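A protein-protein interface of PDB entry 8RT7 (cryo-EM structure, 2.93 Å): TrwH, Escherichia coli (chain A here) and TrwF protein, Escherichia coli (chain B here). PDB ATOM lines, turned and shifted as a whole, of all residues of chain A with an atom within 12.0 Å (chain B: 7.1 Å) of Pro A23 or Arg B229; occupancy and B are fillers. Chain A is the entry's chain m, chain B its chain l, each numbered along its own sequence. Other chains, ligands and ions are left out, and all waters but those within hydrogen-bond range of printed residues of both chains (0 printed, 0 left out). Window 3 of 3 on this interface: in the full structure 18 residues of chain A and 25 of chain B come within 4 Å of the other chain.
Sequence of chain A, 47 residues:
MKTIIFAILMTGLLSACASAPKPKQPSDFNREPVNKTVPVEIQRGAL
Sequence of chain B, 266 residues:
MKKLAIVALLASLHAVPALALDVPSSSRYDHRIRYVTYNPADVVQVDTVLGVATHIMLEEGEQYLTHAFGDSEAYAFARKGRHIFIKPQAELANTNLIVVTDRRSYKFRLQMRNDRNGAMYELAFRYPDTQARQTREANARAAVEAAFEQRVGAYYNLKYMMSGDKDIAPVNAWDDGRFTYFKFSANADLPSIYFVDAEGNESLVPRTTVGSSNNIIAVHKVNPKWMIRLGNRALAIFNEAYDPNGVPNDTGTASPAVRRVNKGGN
The side-chain carboxylate (OD2) of Asp B165 lies within salt-bridge range of the side-chain amino group (NZ) of Lys A24, at 2.7 Å. The backbone carbonyl oxygen (O) of Lys A24 is in hydrogen-bond range of the guanidinium group (NH1) of Arg B229 (2.9 Å).
OD1 of Asp B165 lies within salt-bridge range of NH1 of Arg B233, 3.2 Å away. The side-chain carboxylate of Asp B165 lies within hydrogen-bond range of the backbone NH of Ala B234. The backbone carbonyl oxygen (O) of Ser B192 is in hydrogen-bond range of the backbone NH (N) of Arg B229 (2.8 Å). The backbone carbonyl oxygen (O) of Met B227 is in hydrogen-bond range of the backbone NH (N) of Tyr B194 (2.6 Å). OE1 of Glu B202 lies within salt-bridge range of NH2 of Arg B229 (2.9 Å).
Among the printed residues, merely in contact across the chains: Pro A23 with Arg B229 (3.5 Å), Lys A24 with Asn B232 (3.2 Å), Lys A24 with Arg B233 (3.6 Å), Lys A24 with Ala B234 (3.6 Å), Gln A25 with Glu B202 (3.9 Å), Gln A25 with Arg B229 (3.6 Å), Pro A26 with Met B227 (3.6 Å) and Pro A26 with Ala B234 (3.6 Å).
Ser A19 touches none of the printed residues of chain B. Pro A21 touches none of the printed residues of chain B. Pro A23 touches just one residue of chain B: Arg B229. Printed residues of chain B within 4 Å of Lys A24: Asp B165 (2.7 Å), Arg B229 (2.9 Å), Asn B232 (3.2 Å), Arg B233 (3.6 Å) and Ala B234 (3.6 Å). Of the printed residues of chain B, Pro A26 touches Met B227 and Ala B234. Of the printed residues of chain A, Asp B165 touches Lys A24. No residue of chain A comes within 4 Å of Pro B191. No residue of chain A comes within 4 Å of Ser B192. No residue of chain A comes within 4 Å of Ile B193. Printed residues of chain A within 4 Å of Glu B202: Gln A25 (3.9 Å). Met B227 touches one residue of chain A. No residue of chain A comes within 4 Å of Gly B231. Of the printed residues of chain A, Arg B233 touches Lys A24. Ala B234 touches just these residues of chain A: Lys A24 (3.6 Å) and Pro A26 (3.6 Å). The nearest residue of chain B that does not touch Pro A23 is Glu B202 (5.1 Å). The nearest printed residue of chain B that does not touch Gln A25 is Met B227 (4.7 Å).
Of the 10 printed residues of chain A, 4 touch a printed residue of chain B. Printed residues of chain A that touch a printed residue of chain B: Pro A23, Lys A24, Gln A25 and Pro A26. Hydrophobic or aromatic side chains of chain A within 4 Å of the printed part of chain B: Pro A23 and Pro A26. Along chain A the printed residues that touch a printed residue of chain B span positions 23 to 26. Hydrophobic or aromatic side chains of chain B within 4 Å of the printed part of chain A: Met B227 and Ala B234. Among the printed residues, 10 pairs touch across the chains.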
ATOM      1  N   SER A  19      13.965 -10.529   5.694  1.00  0.00           N
ATOM      2  CA  SER A  19      14.907  -9.468   5.384  1.00  0.00           C
ATOM      3  C   SER A  19      14.988  -9.278   3.877  1.00  0.00           C
ATOM      4  O   SER A  19      14.397 -10.029   3.100  1.00  0.00           O
ATOM      5  CB  SER A  19      16.292  -9.766   5.961  1.00  0.00           C
ATOM      6  OG  SER A  19      16.274  -9.677   7.373  1.00  0.00           O
ATOM      7  N   ALA A  20      15.733  -8.254   3.474  1.00  0.00           N
ATOM      8  CA  ALA A  20      15.792  -7.883   2.071  1.00  0.00           C
ATOM      9  C   ALA A  20      16.616  -8.898   1.289  1.00  0.00           C
ATOM     10  O   ALA A  20      17.688  -9.306   1.741  1.00  0.00           O
ATOM     11  CB  ALA A  20      16.395  -6.495   1.910  1.00  0.00           C
ATOM     12  N   PRO A  21      16.145  -9.328   0.125  1.00  0.00           N
ATOM     13  CA  PRO A  21      16.891 -10.321  -0.647  1.00  0.00           C
ATOM     14  C   PRO A  21      18.243  -9.801  -1.097  1.00  0.00           C
ATOM     15  O   PRO A  21      18.414  -8.622  -1.407  1.00  0.00           O
ATOM     16  CB  PRO A  21      15.980 -10.591  -1.847  1.00  0.00           C
ATOM     17  CG  PRO A  21      15.126  -9.406  -1.942  1.00  0.00           C
ATOM     18  CD  PRO A  21      14.896  -8.950  -0.544  1.00  0.00           C
ATOM     19  N   LYS A  22      19.208 -10.703  -1.127  1.00  0.00           N
ATOM     20  CA  LYS A  22      20.510 -10.411  -1.686  1.00  0.00           C
ATOM     21  C   LYS A  22      20.419 -10.419  -3.204  1.00  0.00           C
ATOM     22  O   LYS A  22      19.509 -11.021  -3.772  1.00  0.00           O
ATOM     23  CB  LYS A  22      21.520 -11.451  -1.221  1.00  0.00           C
ATOM     24  CG  LYS A  22      21.732 -11.508   0.272  1.00  0.00           C
ATOM     25  CD  LYS A  22      22.330 -10.227   0.805  1.00  0.00           C
ATOM     26  CE  LYS A  22      23.793 -10.107   0.444  1.00  0.00           C
ATOM     27  NZ  LYS A  22      24.575  -9.652   1.617  1.00  0.00           N
ATOM     28  N   PRO A  23      21.344  -9.758  -3.890  1.00  0.00           N
ATOM     29  CA  PRO A  23      21.399  -9.900  -5.343  1.00  0.00           C
ATOM     30  C   PRO A  23      21.860 -11.296  -5.716  1.00  0.00           C
ATOM     31  O   PRO A  23      22.416 -12.035  -4.904  1.00  0.00           O
ATOM     32  CB  PRO A  23      22.415  -8.841  -5.774  1.00  0.00           C
ATOM     33  CG  PRO A  23      22.625  -7.995  -4.605  1.00  0.00           C
ATOM     34  CD  PRO A  23      22.372  -8.830  -3.411  1.00  0.00           C
ATOM     35  N   LYS A  24      21.602 -11.660  -6.964  1.00  0.00           N
ATOM     36  CA  LYS A  24      21.948 -12.993  -7.421  1.00  0.00           C
ATOM     37  C   LYS A  24      23.441 -13.237  -7.269  1.00  0.00           C
ATOM     38  O   LYS A  24      24.263 -12.369  -7.565  1.00  0.00           O
ATOM     39  CB  LYS A  24      21.533 -13.178  -8.877  1.00  0.00           C
ATOM     40  CG  LYS A  24      21.771 -14.576  -9.376  1.00  0.00           C
ATOM     41  CD  LYS A  24      22.350 -14.585 -10.760  1.00  0.00           C
ATOM     42  CE  LYS A  24      21.263 -14.592 -11.790  1.00  0.00           C
ATOM     43  NZ  LYS A  24      21.825 -14.913 -13.122  1.00  0.00           N
ATOM     44  N   GLN A  25      23.785 -14.406  -6.780  1.00  0.00           N
ATOM     45  CA  GLN A  25      25.180 -14.815  -6.717  1.00  0.00           C
ATOM     46  C   GLN A  25      25.534 -15.634  -7.946  1.00  0.00           C
ATOM     47  O   GLN A  25      24.850 -16.618  -8.241  1.00  0.00           O
ATOM     48  CB  GLN A  25      25.454 -15.627  -5.466  1.00  0.00           C
ATOM     49  CG  GLN A  25      25.665 -14.794  -4.228  1.00  0.00           C
ATOM     50  CD  GLN A  25      26.882 -13.907  -4.338  1.00  0.00           C
ATOM     51  OE1 GLN A  25      26.776 -12.682  -4.340  1.00  0.00           O
ATOM     52  NE2 GLN A  25      28.052 -14.522  -4.442  1.00  0.00           N
ATOM     53  N   PRO A  26      26.571 -15.261  -8.686  1.00  0.00           N
ATOM     54  CA  PRO A  26      26.931 -16.021  -9.881  1.00  0.00           C
ATOM     55  C   PRO A  26      27.395 -17.423  -9.535  1.00  0.00           C
ATOM     56  O   PRO A  26      28.022 -17.663  -8.500  1.00  0.00           O
ATOM     57  CB  PRO A  26      28.068 -15.196 -10.486  1.00  0.00           C
ATOM     58  CG  PRO A  26      28.662 -14.519  -9.330  1.00  0.00           C
ATOM     59  CD  PRO A  26      27.533 -14.186  -8.416  1.00  0.00           C
ATOM     60  N   SER A  27      27.077 -18.356 -10.424  1.00  0.00           N
ATOM     61  CA  SER A  27      27.514 -19.733 -10.258  1.00  0.00           C
ATOM     62  C   SER A  27      29.009 -19.830 -10.504  1.00  0.00           C
ATOM     63  O   SER A  27      29.524 -19.271 -11.474  1.00  0.00           O
ATOM     64  CB  SER A  27      26.759 -20.639 -11.220  1.00  0.00           C
ATOM     65  OG  SER A  27      27.100 -20.333 -12.559  1.00  0.00           O
ATOM     66  N   ASP A  28      29.709 -20.552  -9.633  1.00  0.00           N
ATOM     67  CA  ASP A  28      31.166 -20.632  -9.680  1.00  0.00           C
ATOM     68  C   ASP A  28      31.644 -21.904 -10.368  1.00  0.00           C
ATOM     69  O   ASP A  28      32.664 -22.484  -9.989  1.00  0.00           O
ATOM     70  CB  ASP A  28      31.741 -20.524  -8.273  1.00  0.00           C
ATOM     71  CG  ASP A  28      33.135 -19.930  -8.255  1.00  0.00           C
ATOM     72  OD1 ASP A  28      33.899 -20.156  -9.217  1.00  0.00           O
ATOM     73  OD2 ASP A  28      33.470 -19.231  -7.277  1.00  0.00           O
ATOM     74  N   ASP B 165      27.161 -15.180 -15.316  1.00  0.00           N
ATOM     75  CA  ASP B 165      26.322 -14.853 -16.466  1.00  0.00           C
ATOM     76  C   ASP B 165      27.210 -14.280 -17.557  1.00  0.00           C
ATOM     77  O   ASP B 165      27.539 -13.095 -17.542  1.00  0.00           O
ATOM     78  CB  ASP B 165      25.231 -13.869 -16.073  1.00  0.00           C
ATOM     79  CG  ASP B 165      24.269 -14.448 -15.068  1.00  0.00           C
ATOM     80  OD1 ASP B 165      23.642 -15.482 -15.366  1.00  0.00           O
ATOM     81  OD2 ASP B 165      24.128 -13.865 -13.978  1.00  0.00           O
ATOM     82  N   ILE B 168      26.884 -10.866 -20.078  1.00  0.00           N
ATOM     83  CA  ILE B 168      27.310  -9.513 -19.761  1.00  0.00           C
ATOM     84  C   ILE B 168      28.825  -9.434 -19.596  1.00  0.00           C
ATOM     85  O   ILE B 168      29.336  -8.461 -19.062  1.00  0.00           O
ATOM     86  CB  ILE B 168      26.589  -8.974 -18.518  1.00  0.00           C
ATOM     87  CG1 ILE B 168      26.807  -9.891 -17.320  1.00  0.00           C
ATOM     88  CG2 ILE B 168      25.116  -8.815 -18.788  1.00  0.00           C
ATOM     89  CD1 ILE B 168      26.399  -9.271 -16.021  1.00  0.00           C
ATOM     90  N   LEU B 190      26.877  -1.431 -21.083  1.00  0.00           N
ATOM     91  CA  LEU B 190      27.960  -1.331 -20.118  1.00  0.00           C
ATOM     92  C   LEU B 190      27.424  -1.606 -18.721  1.00  0.00           C
ATOM     93  O   LEU B 190      26.564  -0.863 -18.240  1.00  0.00           O
ATOM     94  CB  LEU B 190      28.609   0.042 -20.170  1.00  0.00           C
ATOM     95  CG  LEU B 190      29.529   0.342 -21.347  1.00  0.00           C
ATOM     96  CD1 LEU B 190      30.434   1.493 -21.014  1.00  0.00           C
ATOM     97  CD2 LEU B 190      30.336  -0.870 -21.724  1.00  0.00           C
ATOM     98  N   PRO B 191      27.906  -2.633 -18.040  1.00  0.00           N
ATOM     99  CA  PRO B 191      27.339  -2.999 -16.741  1.00  0.00           C
ATOM    100  C   PRO B 191      27.915  -2.203 -15.588  1.00  0.00           C
ATOM    101  O   PRO B 191      28.674  -1.254 -15.783  1.00  0.00           O
ATOM    102  CB  PRO B 191      27.701  -4.477 -16.626  1.00  0.00           C
ATOM    103  CG  PRO B 191      28.955  -4.582 -17.354  1.00  0.00           C
ATOM    104  CD  PRO B 191      28.931  -3.589 -18.469  1.00  0.00           C
ATOM    105  N   SER B 192      27.547  -2.580 -14.375  1.00  0.00           N
ATOM    106  CA  SER B 192      28.068  -1.969 -13.167  1.00  0.00           C
ATOM    107  C   SER B 192      29.057  -2.932 -12.525  1.00  0.00           C
ATOM    108  O   SER B 192      28.805  -4.135 -12.457  1.00  0.00           O
ATOM    109  CB  SER B 192      26.924  -1.635 -12.212  1.00  0.00           C
ATOM    110  OG  SER B 192      27.359  -0.829 -11.141  1.00  0.00           O
ATOM    111  N   ILE B 193      30.192  -2.410 -12.073  1.00  0.00           N
ATOM    112  CA  ILE B 193      31.287  -3.231 -11.575  1.00  0.00           C
ATOM    113  C   ILE B 193      31.530  -2.889 -10.116  1.00  0.00           C
ATOM    114  O   ILE B 193      31.663  -1.714  -9.765  1.00  0.00           O
ATOM    115  CB  ILE B 193      32.566  -3.037 -12.409  1.00  0.00           C
ATOM    116  CG1 ILE B 193      32.311  -3.473 -13.846  1.00  0.00           C
ATOM    117  CG2 ILE B 193      33.715  -3.826 -11.818  1.00  0.00           C
ATOM    118  CD1 ILE B 193      33.270  -2.926 -14.819  1.00  0.00           C
ATOM    119  N   TYR B 194      31.589  -3.915  -9.272  1.00  0.00           N
ATOM    120  CA  TYR B 194      31.692  -3.746  -7.835  1.00  0.00           C
ATOM    121  C   TYR B 194      32.950  -4.407  -7.303  1.00  0.00           C
ATOM    122  O   TYR B 194      33.535  -5.284  -7.930  1.00  0.00           O
ATOM    123  CB  TYR B 194      30.459  -4.311  -7.131  1.00  0.00           C
ATOM    124  CG  TYR B 194      29.240  -3.547  -7.521  1.00  0.00           C
ATOM    125  CD1 TYR B 194      28.989  -2.315  -6.972  1.00  0.00           C
ATOM    126  CD2 TYR B 194      28.384  -4.019  -8.490  1.00  0.00           C
ATOM    127  CE1 TYR B 194      27.914  -1.596  -7.346  1.00  0.00           C
ATOM    128  CE2 TYR B 194      27.298  -3.297  -8.867  1.00  0.00           C
ATOM    129  CZ  TYR B 194      27.075  -2.086  -8.291  1.00  0.00           C
ATOM    130  OH  TYR B 194      25.997  -1.336  -8.646  1.00  0.00           O
ATOM    131  N   GLU B 202      30.427  -6.751  -1.419  1.00  0.00           N
ATOM    132  CA  GLU B 202      30.665  -5.850  -2.530  1.00  0.00           C
ATOM    133  C   GLU B 202      30.560  -4.404  -2.075  1.00  0.00           C
ATOM    134  O   GLU B 202      29.878  -4.088  -1.099  1.00  0.00           O
ATOM    135  CB  GLU B 202      29.672  -6.115  -3.652  1.00  0.00           C
ATOM    136  CG  GLU B 202      29.809  -7.481  -4.255  1.00  0.00           C
ATOM    137  CD  GLU B 202      28.515  -7.982  -4.812  1.00  0.00           C
ATOM    138  OE1 GLU B 202      28.353  -9.212  -4.914  1.00  0.00           O
ATOM    139  OE2 GLU B 202      27.655  -7.147  -5.145  1.00  0.00           O
ATOM    140  N   MET B 227      33.007  -7.916  -9.100  1.00  0.00           N
ATOM    141  CA  MET B 227      31.634  -8.315  -9.366  1.00  0.00           C
ATOM    142  C   MET B 227      31.040  -7.413 -10.431  1.00  0.00           C
ATOM    143  O   MET B 227      31.176  -6.193 -10.364  1.00  0.00           O
ATOM    144  CB  MET B 227      30.785  -8.252  -8.109  1.00  0.00           C
ATOM    145  CG  MET B 227      29.447  -8.929  -8.231  1.00  0.00           C
ATOM    146  SD  MET B 227      29.516 -10.518  -9.050  1.00  0.00           S
ATOM    147  CE  MET B 227      29.920 -11.565  -7.673  1.00  0.00           C
ATOM    148  N   ILE B 228      30.391  -8.018 -11.416  1.00  0.00           N
ATOM    149  CA  ILE B 228      29.759  -7.309 -12.518  1.00  0.00           C
ATOM    150  C   ILE B 228      28.270  -7.613 -12.472  1.00  0.00           C
ATOM    151  O   ILE B 228      27.878  -8.778 -12.385  1.00  0.00           O
ATOM    152  CB  ILE B 228      30.368  -7.725 -13.865  1.00  0.00           C
ATOM    153  CG1 ILE B 228      31.853  -7.393 -13.895  1.00  0.00           C
ATOM    154  CG2 ILE B 228      29.663  -7.047 -14.990  1.00  0.00           C
ATOM    155  CD1 ILE B 228      32.472  -7.563 -15.236  1.00  0.00           C
ATOM    156  N   ARG B 229      27.447  -6.573 -12.495  1.00  0.00           N
ATOM    157  CA  ARG B 229      26.006  -6.722 -12.365  1.00  0.00           C
ATOM    158  C   ARG B 229      25.295  -5.868 -13.398  1.00  0.00           C
ATOM    159  O   ARG B 229      25.655  -4.712 -13.612  1.00  0.00           O
ATOM    160  CB  ARG B 229      25.538  -6.320 -10.978  1.00  0.00           C
ATOM    161  CG  ARG B 229      26.165  -7.116  -9.874  1.00  0.00           C
ATOM    162  CD  ARG B 229      25.414  -6.959  -8.586  1.00  0.00           C
ATOM    163  NE  ARG B 229      25.914  -7.882  -7.586  1.00  0.00           N
ATOM    164  CZ  ARG B 229      25.546  -9.150  -7.498  1.00  0.00           C
ATOM    165  NH1 ARG B 229      24.663  -9.640  -8.346  1.00  0.00           N
ATOM    166  NH2 ARG B 229      26.059  -9.925  -6.561  1.00  0.00           N
ATOM    167  N   LEU B 230      24.277  -6.439 -14.030  1.00  0.00           N
ATOM    168  CA  LEU B 230      23.430  -5.695 -14.960  1.00  0.00           C
ATOM    169  C   LEU B 230      22.010  -6.227 -14.818  1.00  0.00           C
ATOM    170  O   LEU B 230      21.657  -7.237 -15.427  1.00  0.00           O
ATOM    171  CB  LEU B 230      23.923  -5.821 -16.392  1.00  0.00           C
ATOM    172  CG  LEU B 230      23.176  -4.968 -17.410  1.00  0.00           C
ATOM    173  CD1 LEU B 230      22.958  -3.574 -16.882  1.00  0.00           C
ATOM    174  CD2 LEU B 230      23.941  -4.923 -18.688  1.00  0.00           C
ATOM    175  N   GLY B 231      21.196  -5.533 -14.036  1.00  0.00           N
ATOM    176  CA  GLY B 231      19.853  -5.992 -13.783  1.00  0.00           C
ATOM    177  C   GLY B 231      19.878  -7.169 -12.843  1.00  0.00           C
ATOM    178  O   GLY B 231      20.330  -7.046 -11.703  1.00  0.00           O
ATOM    179  N   ASN B 232      19.420  -8.324 -13.312  1.00  0.00           N
ATOM    180  CA  ASN B 232      19.421  -9.547 -12.524  1.00  0.00           C
ATOM    181  C   ASN B 232      20.448 -10.546 -13.042  1.00  0.00           C
ATOM    182  O   ASN B 232      20.325 -11.747 -12.814  1.00  0.00           O
ATOM    183  CB  ASN B 232      18.024 -10.156 -12.506  1.00  0.00           C
ATOM    184  CG  ASN B 232      17.834 -11.151 -11.384  1.00  0.00           C
ATOM    185  OD1 ASN B 232      17.936 -10.809 -10.209  1.00  0.00           O
ATOM    186  ND2 ASN B 232      17.534 -12.392 -11.745  1.00  0.00           N
ATOM    187  N   ARG B 233      21.463 -10.062 -13.745  1.00  0.00           N
ATOM    188  CA  ARG B 233      22.578 -10.878 -14.192  1.00  0.00           C
ATOM    189  C   ARG B 233      23.786 -10.538 -13.339  1.00  0.00           C
ATOM    190  O   ARG B 233      23.934  -9.400 -12.893  1.00  0.00           O
ATOM    191  CB  ARG B 233      22.909 -10.635 -15.665  1.00  0.00           C
ATOM    192  CG  ARG B 233      21.716 -10.457 -16.561  1.00  0.00           C
ATOM    193  CD  ARG B 233      20.885 -11.711 -16.607  1.00  0.00           C
ATOM    194  NE  ARG B 233      21.508 -12.763 -17.393  1.00  0.00           N
ATOM    195  CZ  ARG B 233      21.230 -14.050 -17.247  1.00  0.00           C
ATOM    196  NH1 ARG B 233      21.835 -14.948 -18.002  1.00  0.00           N
ATOM    197  NH2 ARG B 233      20.363 -14.435 -16.328  1.00  0.00           N
ATOM    198  N   ALA B 234      24.640 -11.522 -13.100  1.00  0.00           N
ATOM    199  CA  ALA B 234      25.836 -11.307 -12.307  1.00  0.00           C
ATOM    200  C   ALA B 234      26.971 -12.134 -12.875  1.00  0.00           C
ATOM    201  O   ALA B 234      26.782 -13.297 -13.230  1.00  0.00           O
ATOM    202  CB  ALA B 234      25.606 -11.670 -10.844  1.00  0.00           C
ATOM    203  N   LEU B 235      28.149 -11.530 -12.959  1.00  0.00           N
ATOM    204  CA  LEU B 235      29.352 -12.199 -13.421  1.00  0.00           C
ATOM    205  C   LEU B 235      30.484 -11.866 -12.469  1.00  0.00           C
ATOM    206  O   LEU B 235      30.730 -10.692 -12.188  1.00  0.00           O
ATOM    207  CB  LEU B 235      29.709 -11.758 -14.834  1.00  0.00           C
ATOM    208  CG  LEU B 235      30.953 -12.361 -15.463  1.00  0.00           C
ATOM    209  CD1 LEU B 235      30.650 -13.676 -16.112  1.00  0.00           C
ATOM    210  CD2 LEU B 235      31.509 -11.399 -16.445  1.00  0.00           C
